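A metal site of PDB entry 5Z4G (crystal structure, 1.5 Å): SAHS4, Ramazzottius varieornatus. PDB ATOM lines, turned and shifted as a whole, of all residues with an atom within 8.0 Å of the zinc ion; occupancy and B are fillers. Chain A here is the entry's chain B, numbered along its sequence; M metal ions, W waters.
O of Glu 71 sits at hydrogen-bond distance from NZ of Lys 67, at 2.9 Å.
O of His 73 sits at hydrogen-bond distance from NZ of Lys 67 (3.3 Å).
N of His 75 sits at hydrogen-bond distance from O of Trp 66.
The zinc ion is bound by water W1 (2.0 Å), a ring nitrogen (NE2) of His 75 (2.0 Å), a ring nitrogen (NE2) of His 73 (2.1 Å), the side-chain carboxylate (OE1) of Glu 71 (2.2 Å), water W2 (2.3 Å) and the side-chain carboxylate (OE2) of Glu 71 (2.5 Å).
The zinc ion has six donor atoms within binding distance.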
ATOM      1  N   TRP A  66       0.358  26.578  -7.803  1.00  0.00           N
ATOM      2  CA  TRP A  66       0.517  27.176  -9.121  1.00  0.00           C
ATOM      3  C   TRP A  66       0.001  26.320 -10.258  1.00  0.00           C
ATOM      4  O   TRP A  66      -0.255  25.112 -10.095  1.00  0.00           O
ATOM      5  CB  TRP A  66       1.968  27.670  -9.358  1.00  0.00           C
ATOM      6  CG  TRP A  66       3.017  26.631  -9.605  1.00  0.00           C
ATOM      7  CD1 TRP A  66       3.561  26.293 -10.816  1.00  0.00           C
ATOM      8  CD2 TRP A  66       3.691  25.832  -8.631  1.00  0.00           C
ATOM      9  NE1 TRP A  66       4.523  25.324 -10.652  1.00  0.00           N
ATOM     10  CE2 TRP A  66       4.625  25.019  -9.318  1.00  0.00           C
ATOM     11  CE3 TRP A  66       3.585  25.704  -7.231  1.00  0.00           C
ATOM     12  CZ2 TRP A  66       5.458  24.104  -8.661  1.00  0.00           C
ATOM     13  CZ3 TRP A  66       4.396  24.782  -6.578  1.00  0.00           C
ATOM     14  CH2 TRP A  66       5.321  24.000  -7.295  1.00  0.00           C
ATOM     15  N   LYS A  67      -0.163  26.983 -11.409  1.00  0.00           N
ATOM     16  CA  LYS A  67      -0.706  26.404 -12.627  1.00  0.00           C
ATOM     17  C   LYS A  67       0.175  26.880 -13.786  1.00  0.00           C
ATOM     18  O   LYS A  67       0.333  28.093 -13.999  1.00  0.00           O
ATOM     19  CB  LYS A  67      -2.172  26.873 -12.793  1.00  0.00           C
ATOM     20  CG  LYS A  67      -2.768  26.840 -14.205  1.00  0.00           C
ATOM     21  CD  LYS A  67      -3.688  25.656 -14.419  1.00  0.00           C
ATOM     22  CE  LYS A  67      -2.971  24.486 -15.059  1.00  0.00           C
ATOM     23  NZ  LYS A  67      -3.913  23.361 -15.312  1.00  0.00           N
ATOM     24  N   GLU A  68       0.758  25.937 -14.508  1.00  0.00           N
ATOM     25  CA  GLU A  68       1.524  26.247 -15.721  1.00  0.00           C
ATOM     26  C   GLU A  68       0.529  26.232 -16.882  1.00  0.00           C
ATOM     27  O   GLU A  68      -0.264  25.300 -16.998  1.00  0.00           O
ATOM     28  CB  GLU A  68       2.657  25.231 -15.936  1.00  0.00           C
ATOM     29  CG  GLU A  68       3.531  24.957 -14.714  1.00  0.00           C
ATOM     30  CD  GLU A  68       4.727  25.901 -14.554  1.00  0.00           C
ATOM     31  OE1 GLU A  68       4.723  27.010 -15.128  1.00  0.00           O
ATOM     32  OE2 GLU A  68       5.669  25.514 -13.829  1.00  0.00           O
ATOM     33  N   GLY A  70       0.516  25.631 -20.114  1.00  0.00           N
ATOM     34  CA  GLY A  70       0.488  24.478 -21.028  1.00  0.00           C
ATOM     35  C   GLY A  70       0.125  23.126 -20.444  1.00  0.00           C
ATOM     36  O   GLY A  70       0.063  22.131 -21.174  1.00  0.00           O
ATOM     37  N   GLU A  71      -0.128  23.074 -19.134  1.00  0.00           N
ATOM     38  CA  GLU A  71      -0.393  21.817 -18.421  1.00  0.00           C
ATOM     39  C   GLU A  71      -1.853  21.696 -17.968  1.00  0.00           C
ATOM     40  O   GLU A  71      -2.552  22.696 -17.825  1.00  0.00           O
ATOM     41  CB  GLU A  71       0.537  21.665 -17.216  1.00  0.00           C
ATOM     42  CG  GLU A  71       2.027  21.717 -17.559  1.00  0.00           C
ATOM     43  CD  GLU A  71       2.906  21.342 -16.375  1.00  0.00           C
ATOM     44  OE1 GLU A  71       2.738  21.919 -15.271  1.00  0.00           O
ATOM     45  OE2 GLU A  71       3.764  20.452 -16.539  1.00  0.00           O
ATOM     46  N   ASP A  72      -2.293  20.454 -17.757  1.00  0.00           N
ATOM     47  CA  ASP A  72      -3.677  20.180 -17.344  1.00  0.00           C
ATOM     48  C   ASP A  72      -3.771  19.842 -15.851  1.00  0.00           C
ATOM     49  O   ASP A  72      -4.823  19.380 -15.389  1.00  0.00           O
ATOM     50  CB  ASP A  72      -4.269  19.048 -18.203  1.00  0.00           C
ATOM     51  CG  ASP A  72      -3.567  17.710 -17.997  1.00  0.00           C
ATOM     52  OD1 ASP A  72      -2.377  17.681 -17.586  1.00  0.00           O
ATOM     53  OD2 ASP A  72      -4.217  16.679 -18.255  1.00  0.00           O
ATOM     54  N   HIS A  73      -2.692  20.068 -15.117  1.00  0.00           N
ATOM     55  CA  HIS A  73      -2.643  19.796 -13.691  1.00  0.00           C
ATOM     56  C   HIS A  73      -2.187  21.027 -12.905  1.00  0.00           C
ATOM     57  O   HIS A  73      -1.601  21.953 -13.481  1.00  0.00           O
ATOM     58  CB  HIS A  73      -1.723  18.589 -13.391  1.00  0.00           C
ATOM     59  CG  HIS A  73      -0.303  18.772 -13.843  1.00  0.00           C
ATOM     60  ND1 HIS A  73       0.173  18.225 -15.018  1.00  0.00           N
ATOM     61  CD2 HIS A  73       0.743  19.412 -13.270  1.00  0.00           C
ATOM     62  CE1 HIS A  73       1.455  18.530 -15.151  1.00  0.00           C
ATOM     63  NE2 HIS A  73       1.822  19.254 -14.101  1.00  0.00           N
ATOM     64  N   TYR A  74      -2.466  21.020 -11.599  1.00  0.00           N
ATOM     65  CA  TYR A  74      -2.006  22.047 -10.675  1.00  0.00           C
ATOM     66  C   TYR A  74      -0.854  21.510  -9.869  1.00  0.00           C
ATOM     67  O   TYR A  74      -0.750  20.300  -9.667  1.00  0.00           O
ATOM     68  CB  TYR A  74      -3.136  22.447  -9.723  1.00  0.00           C
ATOM     69  CG  TYR A  74      -4.236  23.203 -10.421  1.00  0.00           C
ATOM     70  CD1 TYR A  74      -5.286  22.523 -11.065  1.00  0.00           C
ATOM     71  CD2 TYR A  74      -4.235  24.612 -10.450  1.00  0.00           C
ATOM     72  CE1 TYR A  74      -6.282  23.225 -11.735  1.00  0.00           C
ATOM     73  CE2 TYR A  74      -5.233  25.312 -11.098  1.00  0.00           C
ATOM     74  CZ  TYR A  74      -6.252  24.619 -11.731  1.00  0.00           C
ATOM     75  OH  TYR A  74      -7.232  25.325 -12.386  1.00  0.00           O
ATOM     76  N   HIS A  75      -0.005  22.411  -9.400  1.00  0.00           N
ATOM     77  CA  HIS A  75       1.097  22.053  -8.522  1.00  0.00           C
ATOM     78  C   HIS A  75       0.871  22.652  -7.143  1.00  0.00           C
ATOM     79  O   HIS A  75       0.328  23.749  -7.009  1.00  0.00           O
ATOM     80  CB  HIS A  75       2.415  22.586  -9.075  1.00  0.00           C
ATOM     81  CG  HIS A  75       3.000  21.775 -10.179  1.00  0.00           C
ATOM     82  ND1 HIS A  75       3.904  20.755  -9.947  1.00  0.00           N
ATOM     83  CD2 HIS A  75       2.838  21.833 -11.519  1.00  0.00           C
ATOM     84  CE1 HIS A  75       4.255  20.213 -11.098  1.00  0.00           C
ATOM     85  NE2 HIS A  75       3.623  20.847 -12.067  1.00  0.00           N
ATOM     86  N   THR A  89       3.696  18.040  -4.918  1.00  0.00           N
ATOM     87  CA  THR A  89       2.958  17.127  -5.779  1.00  0.00           C
ATOM     88  C   THR A  89       2.157  17.892  -6.822  1.00  0.00           C
ATOM     89  O   THR A  89       2.172  19.128  -6.867  1.00  0.00           O
ATOM     90  CB  THR A  89       2.072  16.133  -4.962  1.00  0.00           C
ATOM     91  OG1 THR A  89       1.708  15.003  -5.776  1.00  0.00           O
ATOM     92  CG2 THR A  89       0.810  16.793  -4.381  1.00  0.00           C
ATOM     93  N   SER A  90       1.480  17.143  -7.683  1.00  0.00           N
ATOM     94  CA  SER A  90       0.584  17.711  -8.669  1.00  0.00           C
ATOM     95  C   SER A  90      -0.760  16.994  -8.565  1.00  0.00           C
ATOM     96  O   SER A  90      -0.833  15.856  -8.099  1.00  0.00           O
ATOM     97  CB  SER A  90       1.166  17.581 -10.077  1.00  0.00           C
ATOM     98  OG  SER A  90       1.571  16.253 -10.350  1.00  0.00           O
ATOM     99  N   PHE A  91      -1.812  17.678  -8.989  1.00  0.00           N
ATOM    100  CA  PHE A  91      -3.157  17.110  -8.946  1.00  0.00           C
ATOM    101  C   PHE A  91      -4.027  17.630 -10.077  1.00  0.00           C
ATOM    102  O   PHE A  91      -3.769  18.711 -10.628  1.00  0.00           O
ATOM    103  CB  PHE A  91      -3.831  17.360  -7.564  1.00  0.00           C
ATOM    104  CG  PHE A  91      -4.047  18.803  -7.229  1.00  0.00           C
ATOM    105  CD1 PHE A  91      -3.067  19.534  -6.551  1.00  0.00           C
ATOM    106  CD2 PHE A  91      -5.244  19.452  -7.566  1.00  0.00           C
ATOM    107  CE1 PHE A  91      -3.259  20.871  -6.240  1.00  0.00           C
ATOM    108  CE2 PHE A  91      -5.449  20.785  -7.260  1.00  0.00           C
ATOM    109  CZ  PHE A  91      -4.457  21.488  -6.575  1.00  0.00           C
HETATM  110 ZN    ZN M   1       3.667  20.305 -14.023  1.00  0.00          ZN
HETATM  111  O   HOH W   1       4.712  18.639 -14.029  1.00  0.00           O
HETATM  112  O   HOH W   2       5.548  21.524 -14.384  1.00  0.00           O
